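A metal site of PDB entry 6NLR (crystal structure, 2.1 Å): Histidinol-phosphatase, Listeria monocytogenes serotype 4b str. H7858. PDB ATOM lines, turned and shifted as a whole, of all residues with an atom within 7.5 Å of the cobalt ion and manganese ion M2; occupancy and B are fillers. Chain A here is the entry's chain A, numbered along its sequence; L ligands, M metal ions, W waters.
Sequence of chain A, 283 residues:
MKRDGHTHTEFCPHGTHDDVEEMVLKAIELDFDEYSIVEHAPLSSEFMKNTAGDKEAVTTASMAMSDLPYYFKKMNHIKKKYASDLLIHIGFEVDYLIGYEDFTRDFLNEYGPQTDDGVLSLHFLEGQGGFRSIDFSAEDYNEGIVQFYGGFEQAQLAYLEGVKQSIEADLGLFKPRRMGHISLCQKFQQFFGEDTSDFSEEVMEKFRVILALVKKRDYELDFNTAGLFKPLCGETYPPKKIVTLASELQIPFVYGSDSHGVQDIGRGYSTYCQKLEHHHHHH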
ATOM      1  N   HIS A   6      28.980  -7.052  12.515  1.00  0.00           N
ATOM      2  CA  HIS A   6      27.842  -7.931  12.917  1.00  0.00           C
ATOM      3  C   HIS A   6      26.694  -7.131  13.545  1.00  0.00           C
ATOM      4  O   HIS A   6      26.689  -6.914  14.788  1.00  0.00           O
ATOM      5  CB  HIS A   6      28.391  -9.058  13.791  1.00  0.00           C
ATOM      6  CG  HIS A   6      27.451 -10.196  14.002  1.00  0.00           C
ATOM      7  ND1 HIS A   6      27.902 -11.440  14.411  1.00  0.00           N
ATOM      8  CD2 HIS A   6      26.109 -10.286  13.920  1.00  0.00           C
ATOM      9  CE1 HIS A   6      26.872 -12.249  14.557  1.00  0.00           C
ATOM     10  NE2 HIS A   6      25.751 -11.562  14.257  1.00  0.00           N
ATOM     11  N   THR A   7      25.693  -6.749  12.741  1.00  0.00           N
ATOM     12  CA  THR A   7      24.485  -6.041  13.231  1.00  0.00           C
ATOM     13  C   THR A   7      23.226  -6.603  12.569  1.00  0.00           C
ATOM     14  O   THR A   7      23.318  -7.179  11.457  1.00  0.00           O
ATOM     15  CB  THR A   7      24.558  -4.526  13.008  1.00  0.00           C
ATOM     16  OG1 THR A   7      24.372  -4.253  11.611  1.00  0.00           O
ATOM     17  CG2 THR A   7      25.877  -3.961  13.483  1.00  0.00           C
ATOM     18  N   HIS A   8      22.107  -6.370  13.228  1.00  0.00           N
ATOM     19  CA  HIS A   8      20.747  -6.820  12.851  1.00  0.00           C
ATOM     20  C   HIS A   8      19.842  -5.600  12.695  1.00  0.00           C
ATOM     21  O   HIS A   8      20.311  -4.466  12.945  1.00  0.00           O
ATOM     22  CB  HIS A   8      20.272  -7.872  13.871  1.00  0.00           C
ATOM     23  CG  HIS A   8      21.109  -9.107  13.832  1.00  0.00           C
ATOM     24  ND1 HIS A   8      20.901 -10.098  12.879  1.00  0.00           N
ATOM     25  CD2 HIS A   8      22.188  -9.492  14.543  1.00  0.00           C
ATOM     26  CE1 HIS A   8      21.795 -11.060  13.060  1.00  0.00           C
ATOM     27  NE2 HIS A   8      22.621 -10.682  14.054  1.00  0.00           N
ATOM     28  N   HIS A  14      13.134 -11.537  16.364  1.00  0.00           N
ATOM     29  CA  HIS A  14      13.472 -11.607  17.815  1.00  0.00           C
ATOM     30  C   HIS A  14      14.270 -10.373  18.267  1.00  0.00           C
ATOM     31  O   HIS A  14      14.719 -10.363  19.422  1.00  0.00           O
ATOM     32  CB  HIS A  14      14.237 -12.896  18.140  1.00  0.00           C
ATOM     33  CG  HIS A  14      15.483 -13.114  17.341  1.00  0.00           C
ATOM     34  ND1 HIS A  14      16.723 -12.671  17.728  1.00  0.00           N
ATOM     35  CD2 HIS A  14      15.665 -13.781  16.188  1.00  0.00           C
ATOM     36  CE1 HIS A  14      17.615 -13.034  16.825  1.00  0.00           C
ATOM     37  NE2 HIS A  14      16.989 -13.713  15.870  1.00  0.00           N
ATOM     38  N   VAL A  38      24.080  -7.767   8.649  1.00  0.00           N
ATOM     39  CA  VAL A  38      24.115  -9.212   8.356  1.00  0.00           C
ATOM     40  C   VAL A  38      22.906  -9.859   9.050  1.00  0.00           C
ATOM     41  O   VAL A  38      23.061 -10.548  10.077  1.00  0.00           O
ATOM     42  CB  VAL A  38      25.485  -9.818   8.726  1.00  0.00           C
ATOM     43  CG1 VAL A  38      26.524  -9.426   7.688  1.00  0.00           C
ATOM     44  CG2 VAL A  38      25.953  -9.407  10.115  1.00  0.00           C
ATOM     45  N   GLU A  39      21.748  -9.609   8.483  1.00  0.00           N
ATOM     46  CA  GLU A  39      20.472 -10.098   9.050  1.00  0.00           C
ATOM     47  C   GLU A  39      20.436 -11.639   8.943  1.00  0.00           C
ATOM     48  O   GLU A  39      21.048 -12.207   7.996  1.00  0.00           O
ATOM     49  CB  GLU A  39      19.299  -9.445   8.347  1.00  0.00           C
ATOM     50  CG  GLU A  39      18.007  -9.669   9.089  1.00  0.00           C
ATOM     51  CD  GLU A  39      18.130  -9.318  10.563  1.00  0.00           C
ATOM     52  OE1 GLU A  39      17.977  -8.141  10.894  1.00  0.00           O
ATOM     53  OE2 GLU A  39      18.391 -10.250  11.358  1.00  0.00           O
ATOM     54  N   HIS A  40      19.730 -12.290   9.860  1.00  0.00           N
ATOM     55  CA  HIS A  40      19.532 -13.768   9.796  1.00  0.00           C
ATOM     56  C   HIS A  40      18.908 -14.171   8.459  1.00  0.00           C
ATOM     57  O   HIS A  40      17.829 -13.652   8.115  1.00  0.00           O
ATOM     58  CB  HIS A  40      18.633 -14.220  10.922  1.00  0.00           C
ATOM     59  CG  HIS A  40      19.244 -13.960  12.247  1.00  0.00           C
ATOM     60  ND1 HIS A  40      20.293 -14.726  12.707  1.00  0.00           N
ATOM     61  CD2 HIS A  40      18.964 -13.051  13.191  1.00  0.00           C
ATOM     62  CE1 HIS A  40      20.637 -14.304  13.910  1.00  0.00           C
ATOM     63  NE2 HIS A  40      19.836 -13.268  14.217  1.00  0.00           N
ATOM     64  N   GLU A  93      23.792 -13.080   8.258  1.00  0.00           N
ATOM     65  CA  GLU A  93      24.235 -14.108   9.205  1.00  0.00           C
ATOM     66  C   GLU A  93      23.572 -15.396   8.731  1.00  0.00           C
ATOM     67  O   GLU A  93      22.332 -15.551   8.918  1.00  0.00           O
ATOM     68  CB  GLU A  93      23.896 -13.774  10.650  1.00  0.00           C
ATOM     69  CG  GLU A  93      24.578 -14.741  11.599  1.00  0.00           C
ATOM     70  CD  GLU A  93      24.307 -14.501  13.076  1.00  0.00           C
ATOM     71  OE1 GLU A  93      23.537 -13.570  13.367  1.00  0.00           O
ATOM     72  OE2 GLU A  93      24.872 -15.247  13.914  1.00  0.00           O
ATOM     73  N   ASP A  95      22.922 -19.296   8.803  1.00  0.00           N
ATOM     74  CA  ASP A  95      22.950 -20.512   9.632  1.00  0.00           C
ATOM     75  C   ASP A  95      23.709 -21.594   8.862  1.00  0.00           C
ATOM     76  O   ASP A  95      23.373 -21.846   7.682  1.00  0.00           O
ATOM     77  CB  ASP A  95      21.539 -20.987  10.001  1.00  0.00           C
ATOM     78  CG  ASP A  95      21.028 -20.260  11.218  1.00  0.00           C
ATOM     79  OD1 ASP A  95      21.333 -20.723  12.355  1.00  0.00           O
ATOM     80  OD2 ASP A  95      20.400 -19.218  11.020  1.00  0.00           O
ATOM     81  N   VAL A 119      28.494 -13.533   7.638  1.00  0.00           N
ATOM     82  CA  VAL A 119      28.943 -14.321   8.811  1.00  0.00           C
ATOM     83  C   VAL A 119      28.285 -15.690   8.663  1.00  0.00           C
ATOM     84  O   VAL A 119      27.079 -15.756   8.334  1.00  0.00           O
ATOM     85  CB  VAL A 119      28.577 -13.597  10.111  1.00  0.00           C
ATOM     86  CG1 VAL A 119      28.902 -14.431  11.309  1.00  0.00           C
ATOM     87  CG2 VAL A 119      29.283 -12.243  10.220  1.00  0.00           C
ATOM     88  N   LEU A 120      29.050 -16.755   8.875  1.00  0.00           N
ATOM     89  CA  LEU A 120      28.493 -18.118   8.938  1.00  0.00           C
ATOM     90  C   LEU A 120      28.492 -18.540  10.397  1.00  0.00           C
ATOM     91  O   LEU A 120      29.580 -18.577  10.999  1.00  0.00           O
ATOM     92  CB  LEU A 120      29.340 -19.061   8.073  1.00  0.00           C
ATOM     93  CG  LEU A 120      28.851 -20.503   8.016  1.00  0.00           C
ATOM     94  CD1 LEU A 120      27.532 -20.600   7.291  1.00  0.00           C
ATOM     95  CD2 LEU A 120      29.910 -21.379   7.352  1.00  0.00           C
ATOM     96  N   SER A 121      27.306 -18.815  10.929  1.00  0.00           N
ATOM     97  CA  SER A 121      27.061 -19.056  12.361  1.00  0.00           C
ATOM     98  C   SER A 121      26.379 -20.403  12.578  1.00  0.00           C
ATOM     99  O   SER A 121      25.427 -20.728  11.836  1.00  0.00           O
ATOM    100  CB  SER A 121      26.223 -17.953  12.939  1.00  0.00           C
ATOM    101  OG  SER A 121      26.973 -16.763  12.995  1.00  0.00           O
ATOM    102  N   LEU A 122      26.806 -21.120  13.609  1.00  0.00           N
ATOM    103  CA  LEU A 122      26.114 -22.335  14.100  1.00  0.00           C
ATOM    104  C   LEU A 122      25.199 -21.956  15.287  1.00  0.00           C
ATOM    105  O   LEU A 122      25.732 -21.519  16.343  1.00  0.00           O
ATOM    106  CB  LEU A 122      27.168 -23.376  14.479  1.00  0.00           C
ATOM    107  CG  LEU A 122      26.612 -24.720  14.925  1.00  0.00           C
ATOM    108  CD1 LEU A 122      26.004 -25.464  13.741  1.00  0.00           C
ATOM    109  CD2 LEU A 122      27.690 -25.525  15.601  1.00  0.00           C
ATOM    110  N   HIS A 123      23.901 -22.193  15.149  1.00  0.00           N
ATOM    111  CA  HIS A 123      22.876 -21.871  16.190  1.00  0.00           C
ATOM    112  C   HIS A 123      22.069 -23.108  16.596  1.00  0.00           C
ATOM    113  O   HIS A 123      21.374 -23.029  17.624  1.00  0.00           O
ATOM    114  CB  HIS A 123      21.892 -20.793  15.711  1.00  0.00           C
ATOM    115  CG  HIS A 123      22.500 -19.463  15.397  1.00  0.00           C
ATOM    116  ND1 HIS A 123      22.377 -18.885  14.146  1.00  0.00           N
ATOM    117  CD2 HIS A 123      23.224 -18.600  16.134  1.00  0.00           C
ATOM    118  CE1 HIS A 123      23.000 -17.718  14.136  1.00  0.00           C
ATOM    119  NE2 HIS A 123      23.549 -17.538  15.328  1.00  0.00           N
ATOM    120  N   ASP A 135      21.176 -21.288  21.657  1.00  0.00           N
ATOM    121  CA  ASP A 135      21.231 -19.909  22.237  1.00  0.00           C
ATOM    122  C   ASP A 135      19.854 -19.356  22.623  1.00  0.00           C
ATOM    123  O   ASP A 135      19.800 -18.182  22.945  1.00  0.00           O
ATOM    124  CB  ASP A 135      21.969 -18.969  21.270  1.00  0.00           C
ATOM    125  CG  ASP A 135      21.301 -18.761  19.919  1.00  0.00           C
ATOM    126  OD1 ASP A 135      20.350 -19.479  19.618  1.00  0.00           O
ATOM    127  OD2 ASP A 135      21.746 -17.880  19.185  1.00  0.00           O
ATOM    128  N   GLY A 180      30.984 -16.925  12.767  1.00  0.00           N
ATOM    129  CA  GLY A 180      30.274 -16.238  13.833  1.00  0.00           C
ATOM    130  C   GLY A 180      30.535 -16.820  15.221  1.00  0.00           C
ATOM    131  O   GLY A 180      30.579 -18.044  15.349  1.00  0.00           O
ATOM    132  N   HIS A 181      30.688 -15.934  16.201  1.00  0.00           N
ATOM    133  CA  HIS A 181      30.757 -16.219  17.674  1.00  0.00           C
ATOM    134  C   HIS A 181      31.111 -17.685  17.966  1.00  0.00           C
ATOM    135  O   HIS A 181      30.227 -18.412  18.438  1.00  0.00           O
ATOM    136  CB  HIS A 181      29.443 -15.797  18.345  1.00  0.00           C
ATOM    137  CG  HIS A 181      28.193 -16.159  17.596  1.00  0.00           C
ATOM    138  ND1 HIS A 181      27.942 -17.466  17.177  1.00  0.00           N
ATOM    139  CD2 HIS A 181      27.118 -15.405  17.226  1.00  0.00           C
ATOM    140  CE1 HIS A 181      26.739 -17.494  16.572  1.00  0.00           C
ATOM    141  NE2 HIS A 181      26.220 -16.241  16.579  1.00  0.00           N
ATOM    142  N   LEU A 184      29.776 -20.041  21.261  1.00  0.00           N
ATOM    143  CA  LEU A 184      28.348 -19.789  21.607  1.00  0.00           C
ATOM    144  C   LEU A 184      27.851 -20.836  22.625  1.00  0.00           C
ATOM    145  O   LEU A 184      26.860 -20.572  23.297  1.00  0.00           O
ATOM    146  CB  LEU A 184      27.471 -19.795  20.352  1.00  0.00           C
ATOM    147  CG  LEU A 184      26.041 -19.287  20.567  1.00  0.00           C
ATOM    148  CD1 LEU A 184      26.025 -17.783  20.835  1.00  0.00           C
ATOM    149  CD2 LEU A 184      25.171 -19.597  19.355  1.00  0.00           C
ATOM    150  N   ASP A 222      34.604 -13.551  13.788  1.00  0.00           N
ATOM    151  CA  ASP A 222      33.687 -12.628  14.489  1.00  0.00           C
ATOM    152  C   ASP A 222      34.190 -12.503  15.927  1.00  0.00           C
ATOM    153  O   ASP A 222      34.130 -13.528  16.651  1.00  0.00           O
ATOM    154  CB  ASP A 222      32.277 -13.205  14.358  1.00  0.00           C
ATOM    155  CG  ASP A 222      31.098 -12.461  14.997  1.00  0.00           C
ATOM    156  OD1 ASP A 222      31.059 -11.231  14.873  1.00  0.00           O
ATOM    157  OD2 ASP A 222      30.202 -13.164  15.556  1.00  0.00           O
ATOM    158  N   ASN A 224      32.963 -11.313  18.933  1.00  0.00           N
ATOM    159  CA  ASN A 224      31.555 -10.985  19.252  1.00  0.00           C
ATOM    160  C   ASN A 224      31.417 -10.611  20.735  1.00  0.00           C
ATOM    161  O   ASN A 224      31.708 -11.450  21.616  1.00  0.00           O
ATOM    162  CB  ASN A 224      30.688 -12.123  18.747  1.00  0.00           C
ATOM    163  CG  ASN A 224      29.200 -11.851  18.838  1.00  0.00           C
ATOM    164  OD1 ASN A 224      28.713 -11.344  19.847  1.00  0.00           O
ATOM    165  ND2 ASN A 224      28.498 -12.193  17.768  1.00  0.00           N
ATOM    166  N   ALA A 226      28.575  -9.643  22.291  1.00  0.00           N
ATOM    167  CA  ALA A 226      27.192  -9.841  22.806  1.00  0.00           C
ATOM    168  C   ALA A 226      27.205 -10.602  24.135  1.00  0.00           C
ATOM    169  O   ALA A 226      26.389 -10.299  24.986  1.00  0.00           O
ATOM    170  CB  ALA A 226      26.345 -10.566  21.782  1.00  0.00           C
ATOM    171  N   SER A 257      29.274  -6.356  17.353  1.00  0.00           N
ATOM    172  CA  SER A 257      28.369  -5.989  18.481  1.00  0.00           C
ATOM    173  C   SER A 257      27.213  -6.983  18.576  1.00  0.00           C
ATOM    174  O   SER A 257      26.619  -7.105  19.642  1.00  0.00           O
ATOM    175  CB  SER A 257      27.822  -4.584  18.279  1.00  0.00           C
ATOM    176  OG  SER A 257      27.015  -4.493  17.098  1.00  0.00           O
ATOM    177  N   ASP A 258      26.878  -7.648  17.479  1.00  0.00           N
ATOM    178  CA  ASP A 258      25.629  -8.443  17.358  1.00  0.00           C
ATOM    179  C   ASP A 258      24.420  -7.578  17.750  1.00  0.00           C
ATOM    180  O   ASP A 258      23.515  -8.083  18.443  1.00  0.00           O
ATOM    181  CB  ASP A 258      25.725  -9.719  18.190  1.00  0.00           C
ATOM    182  CG  ASP A 258      25.143 -10.923  17.470  1.00  0.00           C
ATOM    183  OD1 ASP A 258      24.267 -10.717  16.617  1.00  0.00           O
ATOM    184  OD2 ASP A 258      25.623 -12.032  17.733  1.00  0.00           O
ATOM    185  N   SER A 259      24.404  -6.302  17.359  1.00  0.00           N
ATOM    186  CA  SER A 259      23.385  -5.315  17.791  1.00  0.00           C
ATOM    187  C   SER A 259      22.003  -5.709  17.252  1.00  0.00           C
ATOM    188  O   SER A 259      21.899  -5.985  16.033  1.00  0.00           O
ATOM    189  CB  SER A 259      23.774  -3.925  17.356  1.00  0.00           C
ATOM    190  OG  SER A 259      24.866  -3.444  18.151  1.00  0.00           O
ATOM    191  N   HIS A 260      20.997  -5.763  18.126  1.00  0.00           N
ATOM    192  CA  HIS A 260      19.571  -6.008  17.769  1.00  0.00           C
ATOM    193  C   HIS A 260      18.745  -4.736  18.021  1.00  0.00           C
ATOM    194  O   HIS A 260      17.488  -4.788  17.843  1.00  0.00           O
ATOM    195  CB  HIS A 260      19.083  -7.238  18.523  1.00  0.00           C
ATOM    196  CG  HIS A 260      19.581  -8.492  17.898  1.00  0.00           C
ATOM    197  ND1 HIS A 260      20.897  -8.889  17.987  1.00  0.00           N
ATOM    198  CD2 HIS A 260      18.960  -9.437  17.173  1.00  0.00           C
ATOM    199  CE1 HIS A 260      21.054 -10.040  17.352  1.00  0.00           C
ATOM    200  NE2 HIS A 260      19.901 -10.388  16.828  1.00  0.00           N
HETATM  201  S1  LIG L   1      21.875 -13.789  17.149  1.00  0.00           S
HETATM  202  O1  LIG L   1      22.323 -12.824  16.161  1.00  0.00           O
HETATM  203  O2  LIG L   1      20.445 -13.733  17.224  1.00  0.00           O
HETATM  204  O3  LIG L   1      22.438 -13.491  18.456  1.00  0.00           O
HETATM  205  O4  LIG L   1      22.298 -15.115  16.742  1.00  0.00           O
HETATM  206 CO    CO M   1      23.874 -12.207  15.023  1.00  0.00          CO
HETATM  207 MN    MN M   2      24.295 -15.666  15.866  1.00  0.00          MN
HETATM  208 MN    MN M   3      19.536 -12.426  16.167  1.00  0.00          MN
HETATM  209  O   HOH W   1      23.954 -16.081  18.122  1.00  0.00           O
HETATM  210  O   HOH W   2      24.658 -13.927  16.163  1.00  0.00           O
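OG of Ser 121 sits close to OE2 of Glu 93 (2.7 Å).
The backbone NH (N) of Glu 93 lies within hydrogen-bond range of the backbone carbonyl oxygen (O) of Val 38.
The backbone NH (N) of Glu 93 lies within hydrogen-bond range of the backbone carbonyl oxygen (O) of Glu 39.
The side-chain carboxylate of Asp 95 sits at hydrogen-bond distance from a ring nitrogen (ND1) of His 123 (2.8 Å).
ND1 of His 6 is in hydrogen-bond range of ND2 of Asn 224.
The backbone NH of Ser 259 sits at hydrogen-bond distance from the backbone carbonyl oxygen of His 6 (3.5 Å).
O of His 6 is in hydrogen-bond range of OG of Ser 257, 3.4 Å away.
N of His 8 sits at hydrogen-bond distance from O of Ser 259.
Within 4 Å of the cobalt ion: His 6, His 8, Glu 93 and Asp 258.
Within 4 Å of manganese ion M2: Glu 93, His 123 and His 181.
An oxygen (O1) of the ligand binds the cobalt ion.
The cobalt ion is bound by a ring nitrogen (NE2) of His 6 (2.1 Å).
The cobalt ion is bound by the side-chain carboxylate (OE1) of Glu 93 (2.2 Å).
NE2 of His 8 is bound to the cobalt ion, 2.2 Å away.
The cobalt ion is bound by water W2 (2.2 Å).
OD1 of Asp 258 is bound to the cobalt ion (2.2 Å).
The cobalt ion has six donor atoms within binding distance.
Manganese ion M2 is bound by water W2 (1.8 Å), the side-chain carboxylate (OE2) of Glu 93 (2.1 Å), a ring nitrogen (NE2) of His 123 (2.1 Å), a ring nitrogen (NE2) of His 181 (2.1 Å), an oxygen (O4) of the ligand (2.2 Å) and water W1 (2.3 Å).
Manganese ion M2 has six donor atoms within binding distance.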
